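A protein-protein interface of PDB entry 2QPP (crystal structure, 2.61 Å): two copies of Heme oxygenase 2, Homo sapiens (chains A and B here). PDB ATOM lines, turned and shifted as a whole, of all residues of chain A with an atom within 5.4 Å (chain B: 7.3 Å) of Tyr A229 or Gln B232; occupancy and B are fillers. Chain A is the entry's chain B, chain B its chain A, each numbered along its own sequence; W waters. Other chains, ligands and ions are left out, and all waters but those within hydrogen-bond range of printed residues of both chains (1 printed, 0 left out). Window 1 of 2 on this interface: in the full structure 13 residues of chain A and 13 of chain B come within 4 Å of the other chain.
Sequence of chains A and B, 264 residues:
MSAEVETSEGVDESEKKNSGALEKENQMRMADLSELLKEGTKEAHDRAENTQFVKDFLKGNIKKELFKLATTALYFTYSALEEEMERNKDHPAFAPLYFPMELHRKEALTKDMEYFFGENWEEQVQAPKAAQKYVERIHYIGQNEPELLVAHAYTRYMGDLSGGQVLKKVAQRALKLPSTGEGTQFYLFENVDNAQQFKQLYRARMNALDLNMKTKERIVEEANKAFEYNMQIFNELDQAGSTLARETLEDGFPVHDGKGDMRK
Of chain B, only Gln B232 and Asn B235 come within 4 Å of Tyr A229. Gln B232 touches three residues of chain A. Of the printed residues of chain A, Gln B239 touches Lys A133 (3.8 Å) and Gln A232 (3.2 Å). Of the printed residues of chain B, Lys A133 touches Asn B235, Asp B238 and Gln B239. Of the printed residues of chain B, Arg A137 touches Glu B228 (3.0 Å) and Gln B232 (3.5 Å). Leu B237 touches none of the printed residues of chain A. Ala A226 touches none of the printed residues of chain B.
Among the printed residues, pairs that only touch across the chains: Tyr A229 with Asn B235 (3.6 Å), Gln A232 with Asn B235 (3.6 Å) and Lys A133 with Gln B239 (3.8 Å).
The side-chain carboxylate (OE2) of Glu B228 is in salt-bridge range of the guanidinium group (NH1) of Arg A137 (3.0 Å). The guanidinium group (NH1) of Arg A137 sits close to the side-chain amide nitrogen (NE2) of Gln B232 (3.5 Å). The side-chain amino group (NZ) of Lys A225 sits at hydrogen-bond distance from the side-chain amide oxygen (OE1) of Gln B232 (2.7 Å). The side-chain amide nitrogen (NE2) of Gln B232 is in hydrogen-bond range of the side-chain hydroxyl (OH) of Tyr A229, at 3.3 Å. The side-chain amino group of Lys A133 sits at hydrogen-bond distance from the backbone carbonyl oxygen of Asn B235 (3.2 Å). The side-chain carboxylate (OD2) of Asp B238 lies within salt-bridge range of the side-chain amino group (NZ) of Lys A133 (2.7 Å). The side-chain amide nitrogen (NE2) of Gln B239 lies close to the side-chain amide oxygen (OE1) of Gln A232 (3.4 Å).
Water W1 lies within hydrogen-bond range of the side-chain carboxylate (OE2) of Glu B228 and the backbone NH (N) of Arg A137.
Tyr A229 touches Gln B232, but with the chains exchanged Gln A232 does not touch Tyr B229 (12.9 Å). Positions printed for both chains: 130, 133, 226, 227, 228, 229, 230, 231, 232, 233 and 234. Of the 10 pairs that touch across the chains among the printed residues, none has its exchanged pair printed and touching as well.
Of the 18 printed residues of chain B, 5 touch a printed residue of chain A. Of the 16 printed residues of chain A, 5 touch a printed residue of chain B. Printed residues of chain A that touch a printed residue of chain B: Lys A133, Arg A137, Lys A225, Tyr A229 and Gln A232. Hydrophobic or aromatic side chains of chain A within 4 Å of the printed part of chain B: Tyr A229. Among the printed residues, Asp or Glu carboxylates within 4 Å of a Lys or Arg side-chain nitrogen of the other chain: Lys A133 with Asp B238 (2.7 Å) and Arg A137 with Glu B228 (3.0 Å).
The side-chain carboxylate (OE2) of Glu B228 sits at hydrogen-bond distance from the side-chain amide nitrogen (NE2) of Gln B232, 2.9 Å away. OE1 of Gln B232 sits at hydrogen-bond distance from ND2 of Asn B235 (3.3 Å). The side-chain amino group of Lys A133 sits at hydrogen-bond distance from the side-chain amide oxygen of Gln A232, 3.5 Å away.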
ATOM      1  N   ALA A 130      -2.606   2.931  32.593  1.00  0.00           N
ATOM      2  CA  ALA A 130      -1.429   2.121  32.312  1.00  0.00           C
ATOM      3  C   ALA A 130      -1.811   0.665  32.055  1.00  0.00           C
ATOM      4  O   ALA A 130      -1.224   0.003  31.192  1.00  0.00           O
ATOM      5  CB  ALA A 130      -0.425   2.228  33.444  1.00  0.00           C
ATOM      6  N   LYS A 133      -3.272   0.359  28.481  1.00  0.00           N
ATOM      7  CA  LYS A 133      -2.217   0.250  27.485  1.00  0.00           C
ATOM      8  C   LYS A 133      -1.743  -1.190  27.379  1.00  0.00           C
ATOM      9  O   LYS A 133      -1.670  -1.749  26.286  1.00  0.00           O
ATOM     10  CB  LYS A 133      -1.040   1.153  27.843  1.00  0.00           C
ATOM     11  CG  LYS A 133      -1.254   2.616  27.543  1.00  0.00           C
ATOM     12  CD  LYS A 133      -0.127   3.436  28.136  1.00  0.00           C
ATOM     13  CE  LYS A 133      -0.140   4.850  27.606  1.00  0.00           C
ATOM     14  NZ  LYS A 133       1.067   5.590  28.047  1.00  0.00           N
ATOM     15  N   TYR A 134      -1.437  -1.790  28.523  1.00  0.00           N
ATOM     16  CA  TYR A 134      -0.983  -3.176  28.567  1.00  0.00           C
ATOM     17  C   TYR A 134      -2.017  -4.110  27.940  1.00  0.00           C
ATOM     18  O   TYR A 134      -1.669  -4.960  27.117  1.00  0.00           O
ATOM     19  CB  TYR A 134      -0.651  -3.590  30.006  1.00  0.00           C
ATOM     20  CG  TYR A 134       0.070  -4.917  30.135  1.00  0.00           C
ATOM     21  CD1 TYR A 134       0.747  -5.479  29.052  1.00  0.00           C
ATOM     22  CD2 TYR A 134       0.105  -5.595  31.354  1.00  0.00           C
ATOM     23  CE1 TYR A 134       1.416  -6.691  29.172  1.00  0.00           C
ATOM     24  CE2 TYR A 134       0.777  -6.807  31.482  1.00  0.00           C
ATOM     25  CZ  TYR A 134       1.427  -7.349  30.387  1.00  0.00           C
ATOM     26  OH  TYR A 134       2.091  -8.555  30.496  1.00  0.00           O
ATOM     27  N   ARG A 137      -1.992  -3.974  24.181  1.00  0.00           N
ATOM     28  CA  ARG A 137      -0.892  -4.747  23.619  1.00  0.00           C
ATOM     29  C   ARG A 137      -1.190  -6.247  23.615  1.00  0.00           C
ATOM     30  O   ARG A 137      -0.887  -6.937  22.644  1.00  0.00           O
ATOM     31  CB  ARG A 137       0.422  -4.450  24.348  1.00  0.00           C
ATOM     32  CG  ARG A 137       1.645  -5.175  23.790  1.00  0.00           C
ATOM     33  CD  ARG A 137       1.970  -4.763  22.360  1.00  0.00           C
ATOM     34  NE  ARG A 137       3.224  -5.354  21.892  1.00  0.00           N
ATOM     35  CZ  ARG A 137       3.813  -5.060  20.734  1.00  0.00           C
ATOM     36  NH1 ARG A 137       3.275  -4.173  19.905  1.00  0.00           N
ATOM     37  NH2 ARG A 137       4.953  -5.649  20.407  1.00  0.00           N
ATOM     38  N   HIS A 152       4.161 -12.913  27.219  1.00  0.00           N
ATOM     39  CA  HIS A 152       3.269 -12.296  28.191  1.00  0.00           C
ATOM     40  C   HIS A 152       2.821 -13.284  29.265  1.00  0.00           C
ATOM     41  O   HIS A 152       2.681 -12.920  30.434  1.00  0.00           O
ATOM     42  CB  HIS A 152       2.068 -11.665  27.489  1.00  0.00           C
ATOM     43  CG  HIS A 152       2.419 -10.442  26.700  1.00  0.00           C
ATOM     44  ND1 HIS A 152       2.553  -9.198  27.279  1.00  0.00           N
ATOM     45  CD2 HIS A 152       2.690 -10.275  25.384  1.00  0.00           C
ATOM     46  CE1 HIS A 152       2.880  -8.316  26.351  1.00  0.00           C
ATOM     47  NE2 HIS A 152       2.971  -8.945  25.193  1.00  0.00           N
ATOM     48  N   ASN A 224      10.482  -8.033  27.638  1.00  0.00           N
ATOM     49  CA  ASN A 224      11.007  -6.769  28.148  1.00  0.00           C
ATOM     50  C   ASN A 224       9.986  -5.641  28.019  1.00  0.00           C
ATOM     51  O   ASN A 224       9.874  -4.800  28.913  1.00  0.00           O
ATOM     52  CB  ASN A 224      12.325  -6.403  27.468  1.00  0.00           C
ATOM     53  CG  ASN A 224      13.525  -7.037  28.149  1.00  0.00           C
ATOM     54  OD1 ASN A 224      13.720  -6.884  29.355  1.00  0.00           O
ATOM     55  ND2 ASN A 224      14.335  -7.750  27.379  1.00  0.00           N
ATOM     56  N   LYS A 225       9.240  -5.640  26.914  1.00  0.00           N
ATOM     57  CA  LYS A 225       8.098  -4.748  26.748  1.00  0.00           C
ATOM     58  C   LYS A 225       7.070  -4.982  27.849  1.00  0.00           C
ATOM     59  O   LYS A 225       6.570  -4.031  28.453  1.00  0.00           O
ATOM     60  CB  LYS A 225       7.437  -4.952  25.385  1.00  0.00           C
ATOM     61  CG  LYS A 225       7.944  -4.026  24.297  1.00  0.00           C
ATOM     62  CD  LYS A 225       6.936  -3.905  23.158  1.00  0.00           C
ATOM     63  CE  LYS A 225       5.829  -2.907  23.482  1.00  0.00           C
ATOM     64  NZ  LYS A 225       6.311  -1.497  23.437  1.00  0.00           N
ATOM     65  N   ALA A 226       6.772  -6.254  28.104  1.00  0.00           N
ATOM     66  CA  ALA A 226       5.819  -6.645  29.135  1.00  0.00           C
ATOM     67  C   ALA A 226       6.207  -6.079  30.504  1.00  0.00           C
ATOM     68  O   ALA A 226       5.358  -5.558  31.226  1.00  0.00           O
ATOM     69  CB  ALA A 226       5.686  -8.159  29.185  1.00  0.00           C
ATOM     70  N   PHE A 227       7.492  -6.162  30.846  1.00  0.00           N
ATOM     71  CA  PHE A 227       7.990  -5.588  32.096  1.00  0.00           C
ATOM     72  C   PHE A 227       7.784  -4.084  32.142  1.00  0.00           C
ATOM     73  O   PHE A 227       7.385  -3.545  33.174  1.00  0.00           O
ATOM     74  CB  PHE A 227       9.466  -5.930  32.315  1.00  0.00           C
ATOM     75  CG  PHE A 227       9.683  -7.207  33.071  1.00  0.00           C
ATOM     76  CD1 PHE A 227       9.744  -8.430  32.401  1.00  0.00           C
ATOM     77  CD2 PHE A 227       9.814  -7.194  34.456  1.00  0.00           C
ATOM     78  CE1 PHE A 227       9.944  -9.621  33.101  1.00  0.00           C
ATOM     79  CE2 PHE A 227      10.012  -8.378  35.165  1.00  0.00           C
ATOM     80  CZ  PHE A 227      10.075  -9.595  34.485  1.00  0.00           C
ATOM     81  N   GLU A 228       8.042  -3.416  31.019  1.00  0.00           N
ATOM     82  CA  GLU A 228       7.897  -1.966  30.931  1.00  0.00           C
ATOM     83  C   GLU A 228       6.453  -1.528  31.130  1.00  0.00           C
ATOM     84  O   GLU A 228       6.194  -0.475  31.712  1.00  0.00           O
ATOM     85  CB  GLU A 228       8.463  -1.432  29.612  1.00  0.00           C
ATOM     86  CG  GLU A 228       9.986  -1.486  29.532  1.00  0.00           C
ATOM     87  CD  GLU A 228      10.671  -0.881  30.763  1.00  0.00           C
ATOM     88  OE1 GLU A 228      11.383  -1.629  31.474  1.00  0.00           O
ATOM     89  OE2 GLU A 228      10.486   0.334  31.021  1.00  0.00           O
ATOM     90  N   TYR A 229       5.519  -2.344  30.654  1.00  0.00           N
ATOM     91  CA  TYR A 229       4.104  -2.127  30.918  1.00  0.00           C
ATOM     92  C   TYR A 229       3.790  -2.257  32.402  1.00  0.00           C
ATOM     93  O   TYR A 229       2.990  -1.490  32.935  1.00  0.00           O
ATOM     94  CB  TYR A 229       3.242  -3.105  30.120  1.00  0.00           C
ATOM     95  CG  TYR A 229       3.015  -2.691  28.687  1.00  0.00           C
ATOM     96  CD1 TYR A 229       3.471  -3.484  27.635  1.00  0.00           C
ATOM     97  CD2 TYR A 229       2.346  -1.506  28.378  1.00  0.00           C
ATOM     98  CE1 TYR A 229       3.266  -3.105  26.313  1.00  0.00           C
ATOM     99  CE2 TYR A 229       2.137  -1.124  27.059  1.00  0.00           C
ATOM    100  CZ  TYR A 229       2.598  -1.929  26.036  1.00  0.00           C
ATOM    101  OH  TYR A 229       2.396  -1.559  24.732  1.00  0.00           O
ATOM    102  N   ASN A 230       4.419  -3.233  33.055  1.00  0.00           N
ATOM    103  CA  ASN A 230       4.271  -3.429  34.498  1.00  0.00           C
ATOM    104  C   ASN A 230       4.859  -2.270  35.295  1.00  0.00           C
ATOM    105  O   ASN A 230       4.306  -1.878  36.320  1.00  0.00           O
ATOM    106  CB  ASN A 230       4.897  -4.756  34.936  1.00  0.00           C
ATOM    107  CG  ASN A 230       4.072  -5.956  34.510  1.00  0.00           C
ATOM    108  OD1 ASN A 230       2.940  -6.143  34.966  1.00  0.00           O
ATOM    109  ND2 ASN A 230       4.638  -6.783  33.628  1.00  0.00           N
ATOM    110  N   MET A 231       5.975  -1.732  34.803  1.00  0.00           N
ATOM    111  CA  MET A 231       6.617  -0.557  35.387  1.00  0.00           C
ATOM    112  C   MET A 231       5.689   0.647  35.351  1.00  0.00           C
ATOM    113  O   MET A 231       5.517   1.327  36.362  1.00  0.00           O
ATOM    114  CB  MET A 231       7.916  -0.225  34.648  1.00  0.00           C
ATOM    115  CG  MET A 231       9.013  -1.266  34.807  1.00  0.00           C
ATOM    116  SD  MET A 231       9.813  -1.258  36.425  1.00  0.00           S
ATOM    117  CE  MET A 231      10.692   0.314  36.379  1.00  0.00           C
ATOM    118  N   GLN A 232       5.091   0.900  34.189  1.00  0.00           N
ATOM    119  CA  GLN A 232       4.118   1.977  34.035  1.00  0.00           C
ATOM    120  C   GLN A 232       2.976   1.838  35.041  1.00  0.00           C
ATOM    121  O   GLN A 232       2.607   2.812  35.701  1.00  0.00           O
ATOM    122  CB  GLN A 232       3.562   2.022  32.611  1.00  0.00           C
ATOM    123  CG  GLN A 232       4.546   2.489  31.557  1.00  0.00           C
ATOM    124  CD  GLN A 232       3.851   2.964  30.291  1.00  0.00           C
ATOM    125  OE1 GLN A 232       3.347   4.090  30.234  1.00  0.00           O
ATOM    126  NE2 GLN A 232       3.823   2.110  29.268  1.00  0.00           N
ATOM    127  N   ILE A 233       2.438   0.621  35.160  1.00  0.00           N
ATOM    128  CA  ILE A 233       1.369   0.323  36.114  1.00  0.00           C
ATOM    129  C   ILE A 233       1.786   0.653  37.551  1.00  0.00           C
ATOM    130  O   ILE A 233       1.017   1.272  38.291  1.00  0.00           O
ATOM    131  CB  ILE A 233       0.881  -1.151  36.004  1.00  0.00           C
ATOM    132  CG1 ILE A 233       0.252  -1.401  34.625  1.00  0.00           C
ATOM    133  CG2 ILE A 233      -0.119  -1.482  37.122  1.00  0.00           C
ATOM    134  CD1 ILE A 233      -0.039  -2.849  34.314  1.00  0.00           C
ATOM    135  N   PHE A 234       3.005   0.265  37.926  1.00  0.00           N
ATOM    136  CA  PHE A 234       3.506   0.490  39.281  1.00  0.00           C
ATOM    137  C   PHE A 234       3.645   1.971  39.615  1.00  0.00           C
ATOM    138  O   PHE A 234       3.143   2.422  40.646  1.00  0.00           O
ATOM    139  CB  PHE A 234       4.839  -0.232  39.521  1.00  0.00           C
ATOM    140  CG  PHE A 234       4.718  -1.733  39.627  1.00  0.00           C
ATOM    141  CD1 PHE A 234       3.584  -2.326  40.181  1.00  0.00           C
ATOM    142  CD2 PHE A 234       5.753  -2.554  39.194  1.00  0.00           C
ATOM    143  CE1 PHE A 234       3.481  -3.710  40.282  1.00  0.00           C
ATOM    144  CE2 PHE A 234       5.658  -3.938  39.293  1.00  0.00           C
ATOM    145  CZ  PHE A 234       4.522  -4.517  39.840  1.00  0.00           C
ATOM    146  N   LYS B 129      11.738   6.856  19.856  1.00  0.00           N
ATOM    147  CA  LYS B 129      12.112   5.436  19.758  1.00  0.00           C
ATOM    148  C   LYS B 129      11.099   4.583  18.976  1.00  0.00           C
ATOM    149  O   LYS B 129      11.484   3.771  18.131  1.00  0.00           O
ATOM    150  CB  LYS B 129      12.380   4.833  21.145  1.00  0.00           C
ATOM    151  CG  LYS B 129      13.621   5.382  21.853  1.00  0.00           C
ATOM    152  CD  LYS B 129      13.887   4.631  23.154  1.00  0.00           C
ATOM    153  CE  LYS B 129      14.684   5.470  24.162  1.00  0.00           C
ATOM    154  NZ  LYS B 129      16.129   5.641  23.811  1.00  0.00           N
ATOM    155  N   ALA B 130       9.812   4.793  19.247  1.00  0.00           N
ATOM    156  CA  ALA B 130       8.742   4.031  18.600  1.00  0.00           C
ATOM    157  C   ALA B 130       8.562   4.390  17.121  1.00  0.00           C
ATOM    158  O   ALA B 130       8.123   3.559  16.327  1.00  0.00           O
ATOM    159  CB  ALA B 130       7.433   4.207  19.357  1.00  0.00           C
ATOM    160  N   ALA B 131       8.903   5.628  16.765  1.00  0.00           N
ATOM    161  CA  ALA B 131       8.885   6.073  15.373  1.00  0.00           C
ATOM    162  C   ALA B 131      10.012   5.429  14.558  1.00  0.00           C
ATOM    163  O   ALA B 131       9.822   5.099  13.384  1.00  0.00           O
ATOM    164  CB  ALA B 131       8.969   7.584  15.303  1.00  0.00           C
ATOM    165  N   LYS B 133      11.237   2.451  15.013  1.00  0.00           N
ATOM    166  CA  LYS B 133      10.761   1.096  14.726  1.00  0.00           C
ATOM    167  C   LYS B 133       9.861   1.087  13.497  1.00  0.00           C
ATOM    168  O   LYS B 133      10.046   0.268  12.597  1.00  0.00           O
ATOM    169  CB  LYS B 133      10.013   0.507  15.926  1.00  0.00           C
ATOM    170  CG  LYS B 133      10.841   0.336  17.194  1.00  0.00           C
ATOM    171  CD  LYS B 133      11.690  -0.922  17.152  1.00  0.00           C
ATOM    172  CE  LYS B 133      12.394  -1.151  18.484  1.00  0.00           C
ATOM    173  NZ  LYS B 133      13.297  -2.343  18.446  1.00  0.00           N
ATOM    174  N   ALA B 226       0.965  -2.325  11.031  1.00  0.00           N
ATOM    175  CA  ALA B 226       0.988  -0.883  10.798  1.00  0.00           C
ATOM    176  C   ALA B 226       0.229  -0.114  11.878  1.00  0.00           C
ATOM    177  O   ALA B 226       0.756   0.860  12.418  1.00  0.00           O
ATOM    178  CB  ALA B 226       0.450  -0.557   9.410  1.00  0.00           C
ATOM    179  N   PHE B 227      -0.988  -0.565  12.198  1.00  0.00           N
ATOM    180  CA  PHE B 227      -1.797   0.020  13.276  1.00  0.00           C
ATOM    181  C   PHE B 227      -1.068  -0.039  14.615  1.00  0.00           C
ATOM    182  O   PHE B 227      -1.103   0.913  15.392  1.00  0.00           O
ATOM    183  CB  PHE B 227      -3.140  -0.708  13.409  1.00  0.00           C
ATOM    184  CG  PHE B 227      -4.238  -0.142  12.544  1.00  0.00           C
ATOM    185  CD1 PHE B 227      -4.521  -0.700  11.301  1.00  0.00           C
ATOM    186  CD2 PHE B 227      -5.008   0.941  12.985  1.00  0.00           C
ATOM    187  CE1 PHE B 227      -5.539  -0.182  10.505  1.00  0.00           C
ATOM    188  CE2 PHE B 227      -6.028   1.457  12.197  1.00  0.00           C
ATOM    189  CZ  PHE B 227      -6.294   0.897  10.955  1.00  0.00           C
ATOM    190  N   GLU B 228      -0.410  -1.159  14.883  1.00  0.00           N
ATOM    191  CA  GLU B 228       0.252  -1.347  16.169  1.00  0.00           C
ATOM    192  C   GLU B 228       1.488  -0.464  16.315  1.00  0.00           C
ATOM    193  O   GLU B 228       1.797  -0.008  17.417  1.00  0.00           O
ATOM    194  CB  GLU B 228       0.590  -2.820  16.405  1.00  0.00           C
ATOM    195  CG  GLU B 228       1.160  -3.125  17.780  1.00  0.00           C
ATOM    196  CD  GLU B 228       0.205  -2.808  18.916  1.00  0.00           C
ATOM    197  OE1 GLU B 228      -1.004  -2.607  18.664  1.00  0.00           O
ATOM    198  OE2 GLU B 228       0.666  -2.764  20.076  1.00  0.00           O
ATOM    199  N   TYR B 229       2.179  -0.220  15.203  1.00  0.00           N
ATOM    200  CA  TYR B 229       3.290   0.726  15.176  1.00  0.00           C
ATOM    201  C   TYR B 229       2.803   2.114  15.592  1.00  0.00           C
ATOM    202  O   TYR B 229       3.467   2.800  16.376  1.00  0.00           O
ATOM    203  CB  TYR B 229       3.974   0.750  13.798  1.00  0.00           C
ATOM    204  CG  TYR B 229       4.927  -0.409  13.589  1.00  0.00           C
ATOM    205  CD1 TYR B 229       4.691  -1.367  12.607  1.00  0.00           C
ATOM    206  CD2 TYR B 229       6.061  -0.559  14.398  1.00  0.00           C
ATOM    207  CE1 TYR B 229       5.567  -2.444  12.425  1.00  0.00           C
ATOM    208  CE2 TYR B 229       6.935  -1.624  14.229  1.00  0.00           C
ATOM    209  CZ  TYR B 229       6.682  -2.561  13.244  1.00  0.00           C
ATOM    210  OH  TYR B 229       7.549  -3.615  13.089  1.00  0.00           O
ATOM    211  N   ASN B 230       1.627   2.497  15.095  1.00  0.00           N
ATOM    212  CA  ASN B 230       0.960   3.719  15.535  1.00  0.00           C
ATOM    213  C   ASN B 230       0.563   3.665  17.008  1.00  0.00           C
ATOM    214  O   ASN B 230       0.725   4.653  17.733  1.00  0.00           O
ATOM    215  CB  ASN B 230      -0.252   4.049  14.657  1.00  0.00           C
ATOM    216  CG  ASN B 230       0.147   4.470  13.250  1.00  0.00           C
ATOM    217  OD1 ASN B 230       0.294   5.664  12.961  1.00  0.00           O
ATOM    218  ND2 ASN B 230       0.346   3.489  12.369  1.00  0.00           N
ATOM    219  N   MET B 231       0.064   2.513  17.455  1.00  0.00           N
ATOM    220  CA  MET B 231      -0.274   2.330  18.864  1.00  0.00           C
ATOM    221  C   MET B 231       0.936   2.622  19.738  1.00  0.00           C
ATOM    222  O   MET B 231       0.809   3.270  20.774  1.00  0.00           O
ATOM    223  CB  MET B 231      -0.793   0.914  19.141  1.00  0.00           C
ATOM    224  CG  MET B 231      -2.121   0.575  18.470  1.00  0.00           C
ATOM    225  SD  MET B 231      -3.512   1.627  18.952  1.00  0.00           S
ATOM    226  CE  MET B 231      -3.819   1.013  20.610  1.00  0.00           C
ATOM    227  N   GLN B 232       2.108   2.162  19.306  1.00  0.00           N
ATOM    228  CA  GLN B 232       3.328   2.334  20.096  1.00  0.00           C
ATOM    229  C   GLN B 232       3.801   3.785  20.136  1.00  0.00           C
ATOM    230  O   GLN B 232       4.344   4.229  21.146  1.00  0.00           O
ATOM    231  CB  GLN B 232       4.450   1.399  19.622  1.00  0.00           C
ATOM    232  CG  GLN B 232       4.190  -0.085  19.880  1.00  0.00           C
ATOM    233  CD  GLN B 232       3.754  -0.377  21.307  1.00  0.00           C
ATOM    234  OE1 GLN B 232       4.402   0.033  22.271  1.00  0.00           O
ATOM    235  NE2 GLN B 232       2.648  -1.099  21.445  1.00  0.00           N
ATOM    236  N   ILE B 233       3.596   4.509  19.038  1.00  0.00           N
ATOM    237  CA  ILE B 233       3.906   5.935  18.996  1.00  0.00           C
ATOM    238  C   ILE B 233       2.944   6.681  19.921  1.00  0.00           C
ATOM    239  O   ILE B 233       3.375   7.520  20.716  1.00  0.00           O
ATOM    240  CB  ILE B 233       3.873   6.512  17.540  1.00  0.00           C
ATOM    241  CG1 ILE B 233       5.032   5.944  16.714  1.00  0.00           C
ATOM    242  CG2 ILE B 233       3.964   8.037  17.548  1.00  0.00           C
ATOM    243  CD1 ILE B 233       4.826   6.020  15.228  1.00  0.00           C
ATOM    244  N   PHE B 234       1.654   6.350  19.829  1.00  0.00           N
ATOM    245  CA  PHE B 234       0.627   6.922  20.701  1.00  0.00           C
ATOM    246  C   PHE B 234       0.929   6.652  22.167  1.00  0.00           C
ATOM    247  O   PHE B 234       0.780   7.540  23.014  1.00  0.00           O
ATOM    248  CB  PHE B 234      -0.760   6.358  20.376  1.00  0.00           C
ATOM    249  CG  PHE B 234      -1.308   6.787  19.044  1.00  0.00           C
ATOM    250  CD1 PHE B 234      -0.916   7.985  18.452  1.00  0.00           C
ATOM    251  CD2 PHE B 234      -2.251   5.996  18.396  1.00  0.00           C
ATOM    252  CE1 PHE B 234      -1.436   8.376  17.230  1.00  0.00           C
ATOM    253  CE2 PHE B 234      -2.784   6.371  17.177  1.00  0.00           C
ATOM    254  CZ  PHE B 234      -2.380   7.567  16.588  1.00  0.00           C
ATOM    255  N   ASN B 235       1.340   5.416  22.449  1.00  0.00           N
ATOM    256  CA  ASN B 235       1.666   4.968  23.801  1.00  0.00           C
ATOM    257  C   ASN B 235       2.891   5.717  24.344  1.00  0.00           C
ATOM    258  O   ASN B 235       2.896   6.141  25.504  1.00  0.00           O
ATOM    259  CB  ASN B 235       1.807   3.431  23.812  1.00  0.00           C
ATOM    260  CG  ASN B 235       2.562   2.889  25.014  1.00  0.00           C
ATOM    261  OD1 ASN B 235       2.395   3.350  26.147  1.00  0.00           O
ATOM    262  ND2 ASN B 235       3.389   1.872  24.772  1.00  0.00           N
ATOM    263  N   GLU B 236       3.901   5.917  23.496  1.00  0.00           N
ATOM    264  CA  GLU B 236       5.086   6.695  23.880  1.00  0.00           C
ATOM    265  C   GLU B 236       4.771   8.185  24.097  1.00  0.00           C
ATOM    266  O   GLU B 236       5.273   8.788  25.044  1.00  0.00           O
ATOM    267  CB  GLU B 236       6.224   6.525  22.863  1.00  0.00           C
ATOM    268  CG  GLU B 236       7.572   7.098  23.332  1.00  0.00           C
ATOM    269  CD  GLU B 236       8.691   7.000  22.290  1.00  0.00           C
ATOM    270  OE1 GLU B 236       8.395   6.862  21.080  1.00  0.00           O
ATOM    271  OE2 GLU B 236       9.876   7.079  22.687  1.00  0.00           O
ATOM    272  N   LEU B 237       3.942   8.765  23.228  1.00  0.00           N
ATOM    273  CA  LEU B 237       3.563  10.177  23.335  1.00  0.00           C
ATOM    274  C   LEU B 237       2.763  10.489  24.603  1.00  0.00           C
ATOM    275  O   LEU B 237       2.882  11.579  25.165  1.00  0.00           O
ATOM    276  CB  LEU B 237       2.776  10.625  22.100  1.00  0.00           C
ATOM    277  CG  LEU B 237       3.542  10.786  20.783  1.00  0.00           C
ATOM    278  CD1 LEU B 237       2.572  10.867  19.611  1.00  0.00           C
ATOM    279  CD2 LEU B 237       4.456  11.993  20.812  1.00  0.00           C
ATOM    280  N   ASP B 238       1.949   9.528  25.034  1.00  0.00           N
ATOM    281  CA  ASP B 238       1.213   9.606  26.292  1.00  0.00           C
ATOM    282  C   ASP B 238       2.170   9.577  27.491  1.00  0.00           C
ATOM    283  O   ASP B 238       1.990  10.339  28.438  1.00  0.00           O
ATOM    284  CB  ASP B 238       0.192   8.463  26.361  1.00  0.00           C
ATOM    285  CG  ASP B 238      -0.611   8.457  27.651  1.00  0.00           C
ATOM    286  OD1 ASP B 238      -1.767   8.920  27.628  1.00  0.00           O
ATOM    287  OD2 ASP B 238      -0.096   7.975  28.685  1.00  0.00           O
ATOM    288  N   GLN B 239       3.180   8.704  27.440  1.00  0.00           N
ATOM    289  CA  GLN B 239       4.227   8.636  28.471  1.00  0.00           C
ATOM    290  C   GLN B 239       4.910   9.987  28.667  1.00  0.00           C
ATOM    291  O   GLN B 239       5.174  10.397  29.804  1.00  0.00           O
ATOM    292  CB  GLN B 239       5.289   7.595  28.111  1.00  0.00           C
ATOM    293  CG  GLN B 239       4.925   6.148  28.416  1.00  0.00           C
ATOM    294  CD  GLN B 239       6.059   5.176  28.084  1.00  0.00           C
ATOM    295  OE1 GLN B 239       6.505   5.083  26.934  1.00  0.00           O
ATOM    296  NE2 GLN B 239       6.524   4.446  29.094  1.00  0.00           N
HETATM  297  O   HOH W   1      -0.930  -1.541  21.955  1.00  0.00           O
